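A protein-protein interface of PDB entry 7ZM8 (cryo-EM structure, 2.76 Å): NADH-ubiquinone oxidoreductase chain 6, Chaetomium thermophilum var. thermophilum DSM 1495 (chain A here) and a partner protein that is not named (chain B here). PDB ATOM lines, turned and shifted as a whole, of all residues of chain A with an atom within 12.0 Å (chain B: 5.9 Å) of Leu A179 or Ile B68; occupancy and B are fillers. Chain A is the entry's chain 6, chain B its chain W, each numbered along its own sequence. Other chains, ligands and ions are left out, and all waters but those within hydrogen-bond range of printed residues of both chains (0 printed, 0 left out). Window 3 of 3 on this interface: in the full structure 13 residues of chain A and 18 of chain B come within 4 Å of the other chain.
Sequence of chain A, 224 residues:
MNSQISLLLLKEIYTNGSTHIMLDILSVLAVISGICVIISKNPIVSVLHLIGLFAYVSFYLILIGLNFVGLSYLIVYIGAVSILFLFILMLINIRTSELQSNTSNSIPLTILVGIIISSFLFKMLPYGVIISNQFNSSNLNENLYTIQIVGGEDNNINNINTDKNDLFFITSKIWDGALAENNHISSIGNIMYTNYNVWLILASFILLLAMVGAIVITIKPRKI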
ATOM      1  N   LYS A 173      33.215  19.052  -7.012  1.00  0.00           N
ATOM      2  CA  LYS A 173      32.557  18.405  -8.177  1.00  0.00           C
ATOM      3  C   LYS A 173      31.090  18.065  -7.893  1.00  0.00           C
ATOM      4  O   LYS A 173      30.762  17.877  -6.720  1.00  0.00           O
ATOM      5  CB  LYS A 173      33.381  17.156  -8.507  1.00  0.00           C
ATOM      6  CG  LYS A 173      33.182  15.939  -7.622  1.00  0.00           C
ATOM      7  CD  LYS A 173      33.872  14.711  -8.170  1.00  0.00           C
ATOM      8  CE  LYS A 173      35.242  15.001  -8.745  1.00  0.00           C
ATOM      9  NZ  LYS A 173      36.041  13.769  -8.952  1.00  0.00           N
ATOM     10  N   ILE A 174      30.238  17.991  -8.920  1.00  0.00           N
ATOM     11  CA  ILE A 174      28.805  17.579  -8.771  1.00  0.00           C
ATOM     12  C   ILE A 174      28.514  16.522  -9.833  1.00  0.00           C
ATOM     13  O   ILE A 174      29.191  16.533 -10.852  1.00  0.00           O
ATOM     14  CB  ILE A 174      27.825  18.770  -8.892  1.00  0.00           C
ATOM     15  CG1 ILE A 174      26.407  18.415  -8.447  1.00  0.00           C
ATOM     16  CG2 ILE A 174      27.836  19.367 -10.290  1.00  0.00           C
ATOM     17  CD1 ILE A 174      25.474  19.596  -8.462  1.00  0.00           C
ATOM     18  N   TRP A 175      27.513  15.670  -9.620  1.00  0.00           N
ATOM     19  CA  TRP A 175      27.261  14.563 -10.577  1.00  0.00           C
ATOM     20  C   TRP A 175      25.913  14.731 -11.276  1.00  0.00           C
ATOM     21  O   TRP A 175      25.861  14.556 -12.502  1.00  0.00           O
ATOM     22  CB  TRP A 175      27.393  13.216  -9.865  1.00  0.00           C
ATOM     23  CG  TRP A 175      28.805  12.944  -9.453  1.00  0.00           C
ATOM     24  CD1 TRP A 175      29.343  13.083  -8.208  1.00  0.00           C
ATOM     25  CD2 TRP A 175      29.881  12.525 -10.310  1.00  0.00           C
ATOM     26  NE1 TRP A 175      30.670  12.754  -8.225  1.00  0.00           N
ATOM     27  CE2 TRP A 175      31.030  12.412  -9.501  1.00  0.00           C
ATOM     28  CE3 TRP A 175      29.983  12.227 -11.673  1.00  0.00           C
ATOM     29  CZ2 TRP A 175      32.262  12.008 -10.011  1.00  0.00           C
ATOM     30  CZ3 TRP A 175      31.199  11.829 -12.176  1.00  0.00           C
ATOM     31  CH2 TRP A 175      32.319  11.718 -11.354  1.00  0.00           C
ATOM     32  N   ASP A 176      24.866  15.045 -10.521  1.00  0.00           N
ATOM     33  CA  ASP A 176      23.516  15.251 -11.108  1.00  0.00           C
ATOM     34  C   ASP A 176      23.532  16.457 -12.058  1.00  0.00           C
ATOM     35  O   ASP A 176      22.838  16.392 -13.087  1.00  0.00           O
ATOM     36  CB  ASP A 176      22.406  15.203 -10.049  1.00  0.00           C
ATOM     37  CG  ASP A 176      22.690  15.958  -8.762  1.00  0.00           C
ATOM     38  OD1 ASP A 176      23.625  16.777  -8.753  1.00  0.00           O
ATOM     39  OD2 ASP A 176      21.964  15.722  -7.780  1.00  0.00           O
ATOM     40  N   GLY A 177      24.274  17.511 -11.719  1.00  0.00           N
ATOM     41  CA  GLY A 177      24.371  18.707 -12.577  1.00  0.00           C
ATOM     42  C   GLY A 177      25.432  18.587 -13.659  1.00  0.00           C
ATOM     43  O   GLY A 177      25.647  19.581 -14.367  1.00  0.00           O
ATOM     44  N   ALA A 178      26.086  17.431 -13.782  1.00  0.00           N
ATOM     45  CA  ALA A 178      27.076  17.187 -14.854  1.00  0.00           C
ATOM     46  C   ALA A 178      26.575  16.162 -15.863  1.00  0.00           C
ATOM     47  O   ALA A 178      27.384  15.810 -16.723  1.00  0.00           O
ATOM     48  CB  ALA A 178      28.354  16.698 -14.228  1.00  0.00           C
ATOM     49  N   LEU A 179      25.332  15.681 -15.777  1.00  0.00           N
ATOM     50  CA  LEU A 179      24.871  14.567 -16.662  1.00  0.00           C
ATOM     51  C   LEU A 179      25.110  14.884 -18.136  1.00  0.00           C
ATOM     52  O   LEU A 179      25.704  14.057 -18.814  1.00  0.00           O
ATOM     53  CB  LEU A 179      23.388  14.277 -16.417  1.00  0.00           C
ATOM     54  CG  LEU A 179      22.719  13.278 -17.360  1.00  0.00           C
ATOM     55  CD1 LEU A 179      23.210  11.865 -17.099  1.00  0.00           C
ATOM     56  CD2 LEU A 179      21.208  13.336 -17.223  1.00  0.00           C
ATOM     57  N   ALA A 180      24.674  16.049 -18.592  1.00  0.00           N
ATOM     58  CA  ALA A 180      24.797  16.437 -20.003  1.00  0.00           C
ATOM     59  C   ALA A 180      25.243  17.887 -20.056  1.00  0.00           C
ATOM     60  O   ALA A 180      24.478  18.704 -20.542  1.00  0.00           O
ATOM     61  CB  ALA A 180      23.447  16.284 -20.628  1.00  0.00           C
ATOM     62  N   GLU A 181      26.450  18.191 -19.613  1.00  0.00           N
ATOM     63  CA  GLU A 181      26.876  19.607 -19.549  1.00  0.00           C
ATOM     64  C   GLU A 181      26.943  20.199 -20.955  1.00  0.00           C
ATOM     65  O   GLU A 181      27.390  19.507 -21.889  1.00  0.00           O
ATOM     66  CB  GLU A 181      28.154  19.785 -18.727  1.00  0.00           C
ATOM     67  CG  GLU A 181      28.874  21.105 -18.924  1.00  0.00           C
ATOM     68  CD  GLU A 181      30.050  21.046 -19.887  1.00  0.00           C
ATOM     69  OE1 GLU A 181      30.427  19.928 -20.284  1.00  0.00           O
ATOM     70  OE2 GLU A 181      30.579  22.115 -20.244  1.00  0.00           O
ATOM     71  N   ASN A 182      26.533  21.457 -21.083  1.00  0.00           N
ATOM     72  CA  ASN A 182      26.505  22.101 -22.407  1.00  0.00           C
ATOM     73  C   ASN A 182      27.606  23.136 -22.467  1.00  0.00           C
ATOM     74  O   ASN A 182      28.007  23.618 -21.406  1.00  0.00           O
ATOM     75  CB  ASN A 182      25.186  22.817 -22.699  1.00  0.00           C
ATOM     76  CG  ASN A 182      23.969  21.925 -22.690  1.00  0.00           C
ATOM     77  OD1 ASN A 182      24.073  20.712 -22.554  1.00  0.00           O
ATOM     78  ND2 ASN A 182      22.805  22.527 -22.830  1.00  0.00           N
ATOM     79  N   ASN A 183      28.123  23.384 -23.665  1.00  0.00           N
ATOM     80  CA  ASN A 183      29.065  24.508 -23.840  1.00  0.00           C
ATOM     81  C   ASN A 183      28.214  25.767 -23.724  1.00  0.00           C
ATOM     82  O   ASN A 183      27.013  25.668 -23.936  1.00  0.00           O
ATOM     83  CB  ASN A 183      29.736  24.425 -25.201  1.00  0.00           C
ATOM     84  CG  ASN A 183      30.507  23.141 -25.407  1.00  0.00           C
ATOM     85  OD1 ASN A 183      31.146  22.642 -24.484  1.00  0.00           O
ATOM     86  ND2 ASN A 183      30.461  22.607 -26.616  1.00  0.00           N
ATOM     87  N   SER A 187      24.072  26.441 -24.369  1.00  0.00           N
ATOM     88  CA  SER A 187      23.207  27.032 -23.324  1.00  0.00           C
ATOM     89  C   SER A 187      22.557  28.347 -23.788  1.00  0.00           C
ATOM     90  O   SER A 187      21.377  28.540 -23.480  1.00  0.00           O
ATOM     91  CB  SER A 187      24.018  27.194 -22.081  1.00  0.00           C
ATOM     92  OG  SER A 187      24.851  26.070 -21.881  1.00  0.00           O
ATOM     93  N   ASN A 190      19.938  27.328 -26.253  1.00  0.00           N
ATOM     94  CA  ASN A 190      18.752  26.708 -25.624  1.00  0.00           C
ATOM     95  C   ASN A 190      17.722  27.783 -25.288  1.00  0.00           C
ATOM     96  O   ASN A 190      16.537  27.474 -25.356  1.00  0.00           O
ATOM     97  CB  ASN A 190      19.105  25.926 -24.362  1.00  0.00           C
ATOM     98  CG  ASN A 190      19.893  24.656 -24.586  1.00  0.00           C
ATOM     99  OD1 ASN A 190      20.052  24.196 -25.711  1.00  0.00           O
ATOM    100  ND2 ASN A 190      20.394  24.083 -23.507  1.00  0.00           N
ATOM    101  N   LYS B  60      23.794   6.224 -23.482  1.00  0.00           N
ATOM    102  CA  LYS B  60      24.830   6.926 -22.700  1.00  0.00           C
ATOM    103  C   LYS B  60      24.190   7.642 -21.519  1.00  0.00           C
ATOM    104  O   LYS B  60      24.784   7.621 -20.436  1.00  0.00           O
ATOM    105  CB  LYS B  60      25.563   7.919 -23.594  1.00  0.00           C
ATOM    106  CG  LYS B  60      26.854   8.468 -23.011  1.00  0.00           C
ATOM    107  CD  LYS B  60      27.323   9.729 -23.675  1.00  0.00           C
ATOM    108  CE  LYS B  60      28.820   9.745 -23.872  1.00  0.00           C
ATOM    109  NZ  LYS B  60      29.239   8.995 -25.079  1.00  0.00           N
ATOM    110  N   MET B  61      23.032   8.252 -21.710  1.00  0.00           N
ATOM    111  CA  MET B  61      22.405   9.042 -20.630  1.00  0.00           C
ATOM    112  C   MET B  61      21.933   8.093 -19.538  1.00  0.00           C
ATOM    113  O   MET B  61      22.221   8.364 -18.386  1.00  0.00           O
ATOM    114  CB  MET B  61      21.298   9.963 -21.155  1.00  0.00           C
ATOM    115  CG  MET B  61      21.819  11.130 -21.980  1.00  0.00           C
ATOM    116  SD  MET B  61      22.849  12.315 -21.062  1.00  0.00           S
ATOM    117  CE  MET B  61      24.480  11.927 -21.696  1.00  0.00           C
ATOM    118  N   ALA B  63      23.005   5.241 -18.818  1.00  0.00           N
ATOM    119  CA  ALA B  63      24.200   4.662 -18.180  1.00  0.00           C
ATOM    120  C   ALA B  63      24.721   5.603 -17.084  1.00  0.00           C
ATOM    121  O   ALA B  63      25.051   5.092 -16.012  1.00  0.00           O
ATOM    122  CB  ALA B  63      25.223   4.443 -19.254  1.00  0.00           C
ATOM    123  N   ARG B  64      24.762   6.913 -17.335  1.00  0.00           N
ATOM    124  CA  ARG B  64      25.181   7.934 -16.345  1.00  0.00           C
ATOM    125  C   ARG B  64      24.089   8.156 -15.294  1.00  0.00           C
ATOM    126  O   ARG B  64      24.463   8.415 -14.158  1.00  0.00           O
ATOM    127  CB  ARG B  64      25.614   9.222 -17.045  1.00  0.00           C
ATOM    128  CG  ARG B  64      26.813   9.108 -17.965  1.00  0.00           C
ATOM    129  CD  ARG B  64      26.986  10.512 -18.492  1.00  0.00           C
ATOM    130  NE  ARG B  64      28.154  10.640 -19.336  1.00  0.00           N
ATOM    131  CZ  ARG B  64      28.556  11.769 -19.880  1.00  0.00           C
ATOM    132  NH1 ARG B  64      29.645  11.792 -20.621  1.00  0.00           N
ATOM    133  NH2 ARG B  64      27.882  12.879 -19.664  1.00  0.00           N
ATOM    134  N   ILE B  65      22.806   8.005 -15.626  1.00  0.00           N
ATOM    135  CA  ILE B  65      21.701   8.108 -14.629  1.00  0.00           C
ATOM    136  C   ILE B  65      21.800   7.002 -13.571  1.00  0.00           C
ATOM    137  O   ILE B  65      21.656   7.322 -12.386  1.00  0.00           O
ATOM    138  CB  ILE B  65      20.329   8.142 -15.325  1.00  0.00           C
ATOM    139  CG1 ILE B  65      20.044   9.503 -15.960  1.00  0.00           C
ATOM    140  CG2 ILE B  65      19.214   7.698 -14.388  1.00  0.00           C
ATOM    141  CD1 ILE B  65      19.109   9.433 -17.139  1.00  0.00           C
ATOM    142  N   HIS B  66      22.069   5.759 -13.953  1.00  0.00           N
ATOM    143  CA  HIS B  66      22.121   4.637 -12.984  1.00  0.00           C
ATOM    144  C   HIS B  66      23.320   4.802 -12.056  1.00  0.00           C
ATOM    145  O   HIS B  66      23.304   4.212 -10.979  1.00  0.00           O
ATOM    146  CB  HIS B  66      22.100   3.272 -13.659  1.00  0.00           C
ATOM    147  CG  HIS B  66      20.897   2.981 -14.491  1.00  0.00           C
ATOM    148  ND1 HIS B  66      19.641   3.438 -14.168  1.00  0.00           N
ATOM    149  CD2 HIS B  66      20.751   2.244 -15.610  1.00  0.00           C
ATOM    150  CE1 HIS B  66      18.776   3.016 -15.060  1.00  0.00           C
ATOM    151  NE2 HIS B  66      19.431   2.285 -15.954  1.00  0.00           N
ATOM    152  N   LEU B  67      24.294   5.627 -12.446  1.00  0.00           N
ATOM    153  CA  LEU B  67      25.517   5.841 -11.631  1.00  0.00           C
ATOM    154  C   LEU B  67      25.420   7.146 -10.842  1.00  0.00           C
ATOM    155  O   LEU B  67      26.176   7.288  -9.887  1.00  0.00           O
ATOM    156  CB  LEU B  67      26.720   5.884 -12.577  1.00  0.00           C
ATOM    157  CG  LEU B  67      27.140   4.560 -13.206  1.00  0.00           C
ATOM    158  CD1 LEU B  67      28.325   4.766 -14.135  1.00  0.00           C
ATOM    159  CD2 LEU B  67      27.474   3.534 -12.136  1.00  0.00           C
ATOM    160  N   ILE B  68      24.522   8.056 -11.218  1.00  0.00           N
ATOM    161  CA  ILE B  68      24.459   9.403 -10.570  1.00  0.00           C
ATOM    162  C   ILE B  68      24.162   9.286  -9.069  1.00  0.00           C
ATOM    163  O   ILE B  68      24.853   9.977  -8.312  1.00  0.00           O
ATOM    164  CB  ILE B  68      23.472  10.343 -11.300  1.00  0.00           C
ATOM    165  CG1 ILE B  68      24.133  11.087 -12.460  1.00  0.00           C
ATOM    166  CG2 ILE B  68      22.810  11.316 -10.337  1.00  0.00           C
ATOM    167  CD1 ILE B  68      23.168  11.888 -13.296  1.00  0.00           C
ATOM    168  N   PRO B  69      23.211   8.459  -8.576  1.00  0.00           N
ATOM    169  CA  PRO B  69      22.965   8.372  -7.139  1.00  0.00           C
ATOM    170  C   PRO B  69      24.133   7.848  -6.291  1.00  0.00           C
ATOM    171  O   PRO B  69      24.332   8.405  -5.247  1.00  0.00           O
ATOM    172  CB  PRO B  69      21.711   7.493  -7.039  1.00  0.00           C
ATOM    173  CG  PRO B  69      21.050   7.671  -8.377  1.00  0.00           C
ATOM    174  CD  PRO B  69      22.223   7.676  -9.325  1.00  0.00           C
ATOM    175  N   LEU B  70      24.865   6.825  -6.747  1.00  0.00           N
ATOM    176  CA  LEU B  70      26.057   6.354  -5.985  1.00  0.00           C
ATOM    177  C   LEU B  70      27.120   7.441  -5.980  1.00  0.00           C
ATOM    178  O   LEU B  70      27.788   7.614  -4.962  1.00  0.00           O
ATOM    179  CB  LEU B  70      26.599   5.008  -6.476  1.00  0.00           C
ATOM    180  CG  LEU B  70      27.179   4.914  -7.884  1.00  0.00           C
ATOM    181  CD1 LEU B  70      28.697   5.015  -7.857  1.00  0.00           C
ATOM    182  CD2 LEU B  70      26.778   3.590  -8.511  1.00  0.00           C
ATOM    183  N   LEU B  71      27.260   8.147  -7.083  1.00  0.00           N
ATOM    184  CA  LEU B  71      28.348   9.136  -7.156  1.00  0.00           C
ATOM    185  C   LEU B  71      27.986  10.357  -6.318  1.00  0.00           C
ATOM    186  O   LEU B  71      28.889  10.892  -5.682  1.00  0.00           O
ATOM    187  CB  LEU B  71      28.702   9.445  -8.616  1.00  0.00           C
ATOM    188  CG  LEU B  71      29.572   8.410  -9.317  1.00  0.00           C
ATOM    189  CD1 LEU B  71      29.554   8.617 -10.820  1.00  0.00           C
ATOM    190  CD2 LEU B  71      30.987   8.445  -8.776  1.00  0.00           C
ATOM    191  N   GLN B  72      26.724  10.771  -6.332  1.00  0.00           N
ATOM    192  CA  GLN B  72      26.280  11.914  -5.548  1.00  0.00           C
ATOM    193  C   GLN B  72      26.263  11.600  -4.058  1.00  0.00           C
ATOM    194  O   GLN B  72      26.470  12.498  -3.237  1.00  0.00           O
ATOM    195  CB  GLN B  72      24.896  12.354  -6.016  1.00  0.00           C
ATOM    196  CG  GLN B  72      24.465  13.709  -5.509  1.00  0.00           C
ATOM    197  CD  GLN B  72      25.429  14.806  -5.883  1.00  0.00           C
ATOM    198  OE1 GLN B  72      25.733  15.006  -7.053  1.00  0.00           O
ATOM    199  NE2 GLN B  72      25.919  15.527  -4.886  1.00  0.00           N
ATOM    200  N   ALA B  73      26.009  10.345  -3.693  1.00  0.00           N
ATOM    201  CA  ALA B  73      25.974   9.970  -2.285  1.00  0.00           C
ATOM    202  C   ALA B  73      27.352  10.082  -1.652  1.00  0.00           C
ATOM    203  O   ALA B  73      27.485  10.547  -0.516  1.00  0.00           O
ATOM    204  CB  ALA B  73      25.423   8.555  -2.141  1.00  0.00           C
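Of the printed residues of chain B, Leu A179 touches Met B61, Arg B64 and Ile B68.
Of chain A, only Trp A175 (3.9 Å), Asp A176 (3.9 Å) and Leu A179 (3.8 Å) come within 4 Å of Ile B68.
Of chain A, only Leu A179 comes within 4 Å of Met B61.
No residue of chain A comes within 4 Å of Ile B65.
No residue of chain A comes within 4 Å of Leu B67.
No residue of chain A comes within 4 Å of Leu B70.
Gln B72 touches just these residues of chain A: Ile A174, Trp A175 and Asp A176.
Of the printed residues of chain B, Asp A176 touches Ile B68 and Gln B72.
Of the printed residues of chain B, Ile A174 touches Gln B72 (3.7 Å).
Of the printed residues of chain B, Trp A175 touches Ile B68 (3.9 Å), Leu B71 (3.4 Å) and Gln B72 (3.2 Å).
The nearest residue of chain B that does not touch Leu A179 is Ile B65 (4.1 Å).
The nearest residue of chain A that does not touch Ile B68 is Gly A177 (5.9 Å).
The guanidinium group (NH2) of Arg B64 sits at hydrogen-bond distance from the backbone carbonyl oxygen (O) of Leu A179, at 2.6 Å.
The side-chain amide oxygen of Gln B72 sits at hydrogen-bond distance from the backbone NH of Trp A175 (3.2 Å).
The side-chain carboxylate (OD1) of Asp A176 lies close to the side-chain amide oxygen (OE1) of Gln B72, 3.2 Å away.
Ile A174 touches Gln B72.
Ile B68 touches Trp A175.
Trp A175 touches Leu B71.
Ile B68 touches Asp A176.
CE of Met B61 touches O of Leu A179, at 3.8 Å.
CD1 of Leu A179 touches CD1 of Ile B68, 3.8 Å away.
Of the 13 printed residues of chain A, 4 touch a printed residue of chain B.
Hydrophobic or aromatic side chains of chain A that line the printed part of chain B: Ile A174, Trp A175 and Leu A179.
Along chain A the printed residues that touch a printed residue of chain B span positions 174 to 179.
Printed residues of chain B that touch a printed residue of chain A: Met B61, Arg B64, Ile B68, Leu B71 and Gln B72.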
